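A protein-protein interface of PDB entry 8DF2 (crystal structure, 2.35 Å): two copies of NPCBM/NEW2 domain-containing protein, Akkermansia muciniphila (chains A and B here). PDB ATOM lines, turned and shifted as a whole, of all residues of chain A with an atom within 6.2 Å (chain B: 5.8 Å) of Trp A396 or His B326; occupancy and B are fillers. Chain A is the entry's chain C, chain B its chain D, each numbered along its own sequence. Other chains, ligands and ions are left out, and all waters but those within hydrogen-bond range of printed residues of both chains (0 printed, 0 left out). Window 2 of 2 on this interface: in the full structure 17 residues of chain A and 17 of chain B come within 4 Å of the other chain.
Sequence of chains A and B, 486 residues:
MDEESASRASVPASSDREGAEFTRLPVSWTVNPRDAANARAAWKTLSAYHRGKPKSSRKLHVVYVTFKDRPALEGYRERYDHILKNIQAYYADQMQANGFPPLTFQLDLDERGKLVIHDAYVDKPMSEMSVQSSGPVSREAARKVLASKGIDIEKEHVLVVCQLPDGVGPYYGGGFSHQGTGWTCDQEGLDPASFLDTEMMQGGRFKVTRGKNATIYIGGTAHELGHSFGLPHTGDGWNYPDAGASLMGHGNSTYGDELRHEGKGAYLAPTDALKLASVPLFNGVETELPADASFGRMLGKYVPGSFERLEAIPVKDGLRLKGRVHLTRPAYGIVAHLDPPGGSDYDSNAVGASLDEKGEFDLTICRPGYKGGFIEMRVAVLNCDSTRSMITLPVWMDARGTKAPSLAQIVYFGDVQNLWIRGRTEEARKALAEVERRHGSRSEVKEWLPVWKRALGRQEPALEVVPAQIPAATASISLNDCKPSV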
ATOM      1  N   PRO A 314      -3.097 -15.418  11.233  1.00  0.00           N
ATOM      2  CA  PRO A 314      -2.022 -14.428  11.076  1.00  0.00           C
ATOM      3  C   PRO A 314      -0.943 -14.585  12.138  1.00  0.00           C
ATOM      4  O   PRO A 314      -1.217 -14.948  13.282  1.00  0.00           O
ATOM      5  CB  PRO A 314      -2.747 -13.080  11.219  1.00  0.00           C
ATOM      6  CG  PRO A 314      -3.927 -13.384  12.065  1.00  0.00           C
ATOM      7  CD  PRO A 314      -4.350 -14.806  11.710  1.00  0.00           C
ATOM      8  N   GLY A 372       3.092  -3.905   1.885  1.00  0.00           N
ATOM      9  CA  GLY A 372       2.033  -3.789   0.899  1.00  0.00           C
ATOM     10  C   GLY A 372       0.631  -4.032   1.431  1.00  0.00           C
ATOM     11  O   GLY A 372      -0.335  -3.718   0.728  1.00  0.00           O
ATOM     12  N   GLY A 373       0.493  -4.588   2.633  1.00  0.00           N
ATOM     13  CA  GLY A 373      -0.829  -4.875   3.151  1.00  0.00           C
ATOM     14  C   GLY A 373      -1.443  -6.079   2.467  1.00  0.00           C
ATOM     15  O   GLY A 373      -1.292  -7.211   2.941  1.00  0.00           O
ATOM     16  N   PHE A 374      -2.137  -5.857   1.352  1.00  0.00           N
ATOM     17  CA  PHE A 374      -2.735  -6.970   0.629  1.00  0.00           C
ATOM     18  C   PHE A 374      -1.657  -7.829  -0.016  1.00  0.00           C
ATOM     19  O   PHE A 374      -0.654  -7.321  -0.523  1.00  0.00           O
ATOM     20  CB  PHE A 374      -3.707  -6.483  -0.449  1.00  0.00           C
ATOM     21  CG  PHE A 374      -4.091  -7.559  -1.437  1.00  0.00           C
ATOM     22  CD1 PHE A 374      -4.944  -8.590  -1.061  1.00  0.00           C
ATOM     23  CD2 PHE A 374      -3.571  -7.563  -2.725  1.00  0.00           C
ATOM     24  CE1 PHE A 374      -5.288  -9.593  -1.955  1.00  0.00           C
ATOM     25  CE2 PHE A 374      -3.909  -8.563  -3.621  1.00  0.00           C
ATOM     26  CZ  PHE A 374      -4.772  -9.579  -3.238  1.00  0.00           C
ATOM     27  N   ILE A 375      -1.878  -9.137  -0.003  1.00  0.00           N
ATOM     28  CA  ILE A 375      -0.989 -10.078  -0.670  1.00  0.00           C
ATOM     29  C   ILE A 375      -1.809 -11.286  -1.106  1.00  0.00           C
ATOM     30  O   ILE A 375      -2.751 -11.699  -0.421  1.00  0.00           O
ATOM     31  CB  ILE A 375       0.196 -10.468   0.238  1.00  0.00           C
ATOM     32  CG1 ILE A 375       1.209 -11.317  -0.535  1.00  0.00           C
ATOM     33  CG2 ILE A 375      -0.299 -11.162   1.487  1.00  0.00           C
ATOM     34  CD1 ILE A 375       2.654 -10.995  -0.195  1.00  0.00           C
ATOM     35  N   PRO A 394      -7.404 -14.120  -0.841  1.00  0.00           N
ATOM     36  CA  PRO A 394      -6.932 -12.749  -0.631  1.00  0.00           C
ATOM     37  C   PRO A 394      -6.648 -12.475   0.839  1.00  0.00           C
ATOM     38  O   PRO A 394      -7.532 -12.612   1.697  1.00  0.00           O
ATOM     39  CB  PRO A 394      -8.091 -11.902  -1.164  1.00  0.00           C
ATOM     40  CG  PRO A 394      -9.322 -12.785  -1.012  1.00  0.00           C
ATOM     41  CD  PRO A 394      -8.873 -14.209  -0.802  1.00  0.00           C
ATOM     42  N   VAL A 395      -5.414 -12.088   1.137  1.00  0.00           N
ATOM     43  CA  VAL A 395      -4.923 -11.994   2.504  1.00  0.00           C
ATOM     44  C   VAL A 395      -4.412 -10.582   2.775  1.00  0.00           C
ATOM     45  O   VAL A 395      -3.831  -9.933   1.895  1.00  0.00           O
ATOM     46  CB  VAL A 395      -3.812 -13.033   2.752  1.00  0.00           C
ATOM     47  CG1 VAL A 395      -3.339 -12.986   4.206  1.00  0.00           C
ATOM     48  CG2 VAL A 395      -4.304 -14.408   2.375  1.00  0.00           C
ATOM     49  N   TRP A 396      -4.642 -10.106   3.994  1.00  0.00           N
ATOM     50  CA  TRP A 396      -4.019  -8.889   4.488  1.00  0.00           C
ATOM     51  C   TRP A 396      -2.973  -9.270   5.524  1.00  0.00           C
ATOM     52  O   TRP A 396      -3.269 -10.021   6.462  1.00  0.00           O
ATOM     53  CB  TRP A 396      -5.045  -7.939   5.098  1.00  0.00           C
ATOM     54  CG  TRP A 396      -4.405  -6.714   5.656  1.00  0.00           C
ATOM     55  CD1 TRP A 396      -3.881  -6.560   6.906  1.00  0.00           C
ATOM     56  CD2 TRP A 396      -4.207  -5.465   4.980  1.00  0.00           C
ATOM     57  NE1 TRP A 396      -3.374  -5.294   7.053  1.00  0.00           N
ATOM     58  CE2 TRP A 396      -3.560  -4.599   5.888  1.00  0.00           C
ATOM     59  CE3 TRP A 396      -4.515  -4.992   3.701  1.00  0.00           C
ATOM     60  CZ2 TRP A 396      -3.222  -3.290   5.557  1.00  0.00           C
ATOM     61  CZ3 TRP A 396      -4.171  -3.688   3.374  1.00  0.00           C
ATOM     62  CH2 TRP A 396      -3.534  -2.856   4.298  1.00  0.00           C
ATOM     63  N   MET A 397      -1.768  -8.727   5.371  1.00  0.00           N
ATOM     64  CA  MET A 397      -0.611  -9.129   6.158  1.00  0.00           C
ATOM     65  C   MET A 397       0.136  -7.892   6.641  1.00  0.00           C
ATOM     66  O   MET A 397       0.424  -6.990   5.848  1.00  0.00           O
ATOM     67  CB  MET A 397       0.303 -10.019   5.309  1.00  0.00           C
ATOM     68  CG  MET A 397       1.501 -10.578   6.023  1.00  0.00           C
ATOM     69  SD  MET A 397       2.519 -11.528   4.890  1.00  0.00           S
ATOM     70  CE  MET A 397       1.967 -13.168   5.305  1.00  0.00           C
ATOM     71  N   ASP A 398       0.450  -7.851   7.933  1.00  0.00           N
ATOM     72  CA  ASP A 398       1.275  -6.782   8.495  1.00  0.00           C
ATOM     73  C   ASP A 398       1.972  -7.321   9.739  1.00  0.00           C
ATOM     74  O   ASP A 398       1.933  -8.523  10.024  1.00  0.00           O
ATOM     75  CB  ASP A 398       0.431  -5.535   8.803  1.00  0.00           C
ATOM     76  CG  ASP A 398      -0.793  -5.854   9.646  1.00  0.00           C
ATOM     77  OD1 ASP A 398      -0.943  -7.028  10.028  1.00  0.00           O
ATOM     78  OD2 ASP A 398      -1.611  -4.946   9.923  1.00  0.00           O
ATOM     79  N   GLY B 305     -11.735  -7.776  -1.780  1.00  0.00           N
ATOM     80  CA  GLY B 305     -11.639  -7.822  -0.339  1.00  0.00           C
ATOM     81  C   GLY B 305     -10.507  -8.747   0.059  1.00  0.00           C
ATOM     82  O   GLY B 305      -9.930  -9.449  -0.778  1.00  0.00           O
ATOM     83  N   SER B 306     -10.194  -8.738   1.348  1.00  0.00           N
ATOM     84  CA  SER B 306      -9.128  -9.590   1.851  1.00  0.00           C
ATOM     85  C   SER B 306      -9.400  -9.932   3.306  1.00  0.00           C
ATOM     86  O   SER B 306     -10.091  -9.200   4.021  1.00  0.00           O
ATOM     87  CB  SER B 306      -7.762  -8.912   1.717  1.00  0.00           C
ATOM     88  OG  SER B 306      -7.740  -7.714   2.472  1.00  0.00           O
ATOM     89  N   PHE B 307      -8.793 -11.031   3.748  1.00  0.00           N
ATOM     90  CA  PHE B 307      -8.954 -11.539   5.100  1.00  0.00           C
ATOM     91  C   PHE B 307      -7.624 -11.478   5.841  1.00  0.00           C
ATOM     92  O   PHE B 307      -6.574 -11.821   5.285  1.00  0.00           O
ATOM     93  CB  PHE B 307      -9.472 -12.986   5.094  1.00  0.00           C
ATOM     94  CG  PHE B 307     -10.882 -13.129   4.578  1.00  0.00           C
ATOM     95  CD1 PHE B 307     -11.131 -13.203   3.220  1.00  0.00           C
ATOM     96  CD2 PHE B 307     -11.956 -13.209   5.455  1.00  0.00           C
ATOM     97  CE1 PHE B 307     -12.426 -13.334   2.739  1.00  0.00           C
ATOM     98  CE2 PHE B 307     -13.255 -13.344   4.977  1.00  0.00           C
ATOM     99  CZ  PHE B 307     -13.487 -13.404   3.618  1.00  0.00           C
ATOM    100  N   GLU B 308      -7.675 -11.029   7.095  1.00  0.00           N
ATOM    101  CA  GLU B 308      -6.523 -11.176   7.975  1.00  0.00           C
ATOM    102  C   GLU B 308      -6.484 -12.561   8.608  1.00  0.00           C
ATOM    103  O   GLU B 308      -5.402 -13.074   8.904  1.00  0.00           O
ATOM    104  CB  GLU B 308      -6.546 -10.108   9.071  1.00  0.00           C
ATOM    105  CG  GLU B 308      -7.079  -8.764   8.629  1.00  0.00           C
ATOM    106  CD  GLU B 308      -6.829  -7.652   9.646  1.00  0.00           C
ATOM    107  OE1 GLU B 308      -6.661  -7.949  10.850  1.00  0.00           O
ATOM    108  OE2 GLU B 308      -6.809  -6.470   9.236  1.00  0.00           O
ATOM    109  N   ARG B 324     -11.411 -12.907  10.423  1.00  0.00           N
ATOM    110  CA  ARG B 324     -11.328 -11.454  10.517  1.00  0.00           C
ATOM    111  C   ARG B 324     -11.190 -10.897   9.110  1.00  0.00           C
ATOM    112  O   ARG B 324     -10.181 -11.144   8.439  1.00  0.00           O
ATOM    113  CB  ARG B 324     -10.154 -11.012  11.388  1.00  0.00           C
ATOM    114  CG  ARG B 324     -10.150  -9.527  11.700  1.00  0.00           C
ATOM    115  CD  ARG B 324      -9.065  -9.189  12.719  1.00  0.00           C
ATOM    116  NE  ARG B 324      -9.003  -7.757  12.982  1.00  0.00           N
ATOM    117  CZ  ARG B 324      -8.367  -7.203  14.006  1.00  0.00           C
ATOM    118  NH1 ARG B 324      -7.720  -7.936  14.900  1.00  0.00           N
ATOM    119  NH2 ARG B 324      -8.383  -5.880  14.139  1.00  0.00           N
ATOM    120  N   VAL B 325     -12.221 -10.179   8.662  1.00  0.00           N
ATOM    121  CA  VAL B 325     -12.143  -9.434   7.413  1.00  0.00           C
ATOM    122  C   VAL B 325     -11.262  -8.212   7.622  1.00  0.00           C
ATOM    123  O   VAL B 325     -11.399  -7.497   8.622  1.00  0.00           O
ATOM    124  CB  VAL B 325     -13.547  -9.017   6.944  1.00  0.00           C
ATOM    125  CG1 VAL B 325     -13.458  -8.168   5.670  1.00  0.00           C
ATOM    126  CG2 VAL B 325     -14.459 -10.240   6.746  1.00  0.00           C
ATOM    127  N   HIS B 326     -10.353  -7.958   6.687  1.00  0.00           N
ATOM    128  CA  HIS B 326      -9.660  -6.678   6.686  1.00  0.00           C
ATOM    129  C   HIS B 326     -10.580  -5.609   6.107  1.00  0.00           C
ATOM    130  O   HIS B 326     -10.970  -5.683   4.938  1.00  0.00           O
ATOM    131  CB  HIS B 326      -8.368  -6.740   5.886  1.00  0.00           C
ATOM    132  CG  HIS B 326      -7.672  -5.424   5.824  1.00  0.00           C
ATOM    133  ND1 HIS B 326      -6.968  -4.907   6.891  1.00  0.00           N
ATOM    134  CD2 HIS B 326      -7.607  -4.493   4.841  1.00  0.00           C
ATOM    135  CE1 HIS B 326      -6.488  -3.721   6.563  1.00  0.00           C
ATOM    136  NE2 HIS B 326      -6.855  -3.451   5.323  1.00  0.00           N
ATOM    137  N   LEU B 327     -10.904  -4.602   6.912  1.00  0.00           N
ATOM    138  CA  LEU B 327     -11.865  -3.576   6.515  1.00  0.00           C
ATOM    139  C   LEU B 327     -11.136  -2.516   5.699  1.00  0.00           C
ATOM    140  O   LEU B 327     -10.500  -1.614   6.239  1.00  0.00           O
ATOM    141  CB  LEU B 327     -12.546  -2.963   7.734  1.00  0.00           C
ATOM    142  CG  LEU B 327     -13.451  -3.807   8.643  1.00  0.00           C
ATOM    143  CD1 LEU B 327     -14.258  -4.867   7.901  1.00  0.00           C
ATOM    144  CD2 LEU B 327     -12.612  -4.437   9.726  1.00  0.00           C
ATOM    145  N   THR B 328     -11.191  -2.657   4.374  1.00  0.00           N
ATOM    146  CA  THR B 328     -10.769  -1.563   3.503  1.00  0.00           C
ATOM    147  C   THR B 328     -11.812  -0.448   3.475  1.00  0.00           C
ATOM    148  O   THR B 328     -11.483   0.715   3.222  1.00  0.00           O
ATOM    149  CB  THR B 328     -10.518  -2.090   2.086  1.00  0.00           C
ATOM    150  OG1 THR B 328     -11.762  -2.505   1.498  1.00  0.00           O
ATOM    151  CG2 THR B 328      -9.567  -3.281   2.114  1.00  0.00           C
ATOM    152  N   ARG B 329     -13.062  -0.785   3.743  1.00  0.00           N
ATOM    153  CA  ARG B 329     -14.172   0.146   3.794  1.00  0.00           C
ATOM    154  C   ARG B 329     -15.113  -0.329   4.889  1.00  0.00           C
ATOM    155  O   ARG B 329     -15.039  -1.485   5.318  1.00  0.00           O
ATOM    156  CB  ARG B 329     -14.902   0.213   2.443  1.00  0.00           C
ATOM    157  CG  ARG B 329     -15.469  -1.126   1.980  1.00  0.00           C
ATOM    158  CD  ARG B 329     -15.748  -1.142   0.483  1.00  0.00           C
ATOM    159  NE  ARG B 329     -14.535  -1.360  -0.295  1.00  0.00           N
ATOM    160  CZ  ARG B 329     -14.281  -0.771  -1.455  1.00  0.00           C
ATOM    161  NH1 ARG B 329     -15.137   0.079  -2.000  1.00  0.00           N
ATOM    162  NH2 ARG B 329     -13.137  -1.034  -2.081  1.00  0.00           N
ATOM    163  N   GLY B 359     -13.926  -6.319  12.235  1.00  0.00           N
ATOM    164  CA  GLY B 359     -14.119  -7.276  11.161  1.00  0.00           C
ATOM    165  C   GLY B 359     -14.232  -8.729  11.576  1.00  0.00           C
ATOM    166  O   GLY B 359     -14.149  -9.611  10.711  1.00  0.00           O
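The backbone NH (N) of Ile A375 lies within hydrogen-bond range of the backbone carbonyl oxygen (O) of Val A395, 2.8 Å away.
The indole nitrogen (NE1) of Trp A396 is in hydrogen-bond range of the side-chain carboxylate (OD2) of Asp A398 (3.4 Å).
The backbone NH of His B326 lies within hydrogen-bond range of the backbone carbonyl oxygen of Ser B306, at 3.0 Å.
The guanidinium group of Arg B324 is in salt-bridge range of the side-chain carboxylate of Glu B308.
OE2 of Glu B308 lies within hydrogen-bond range of ND1 of His B326.
Of chain A, only Trp A396 comes within 4 Å of His B326.
Of the printed residues of chain A, Ser B306 touches Phe A374 (3.97 Å), Pro A394 (3.4 Å), Val A395 (3.9 Å) and Trp A396 (3.8 Å).
Of the printed residues of chain A, Gly B305 touches Pro A394.
Printed residues of chain B within 4 Å of Phe A374: Ser B306 (3.97 Å).
Gly A373 touches none of the printed residues of chain B.
Arg B329 touches none of the printed residues of chain A.
The nearest residue of chain B that does not touch Trp A396 is Thr B328 (5.6 Å).
The nearest printed residue of chain A that does not touch His B326 is Asp A398 (6.0 Å).
The nearest printed residue of chain B that does not touch Pro A394 is Glu B308 (5.6 Å).
Of the 10 printed residues of chain A, 5 touch a printed residue of chain B.
Along chain A the printed residues that touch a printed residue of chain B span positions 314 to 396.
Of the 11 printed residues of chain B, 5 touch a printed residue of chain A.
Hydrophobic or aromatic side chains of chain B within 4 Å of the printed part of chain A: Phe B307 and His B326.
Among the printed residues, no Asp or Glu carboxylate lies within 4 Å of a Lys or Arg side-chain nitrogen of the other chain.
O of Glu B308 touches CD of Pro A314, 3.5 Å away.
CB of Ser B306 touches CD1 of Phe A374, at 3.97 Å.
Gly B305 touches Pro A394.
Pro A394 touches Ser B306.
CB of Ser B306 touches C of Val A395 (3.9 Å).
O of Phe B307 touches CA of Val A395, at 3.2 Å.
CB of Trp A396 touches OG of Ser B306 (3.8 Å).
OE2 of Glu B308 touches CD1 of Trp A396 (3.7 Å).
His B326 touches Trp A396 (CE1 to CE2, 3.1 Å).
No position is printed for both chains.
The backbone NH (N) of Phe B307 sits at hydrogen-bond distance from the backbone carbonyl oxygen (O) of Pro A394, 2.9 Å away.
The backbone NH (N) of Trp A396 is in hydrogen-bond range of the backbone carbonyl oxygen (O) of Phe B307 (2.9 Å).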
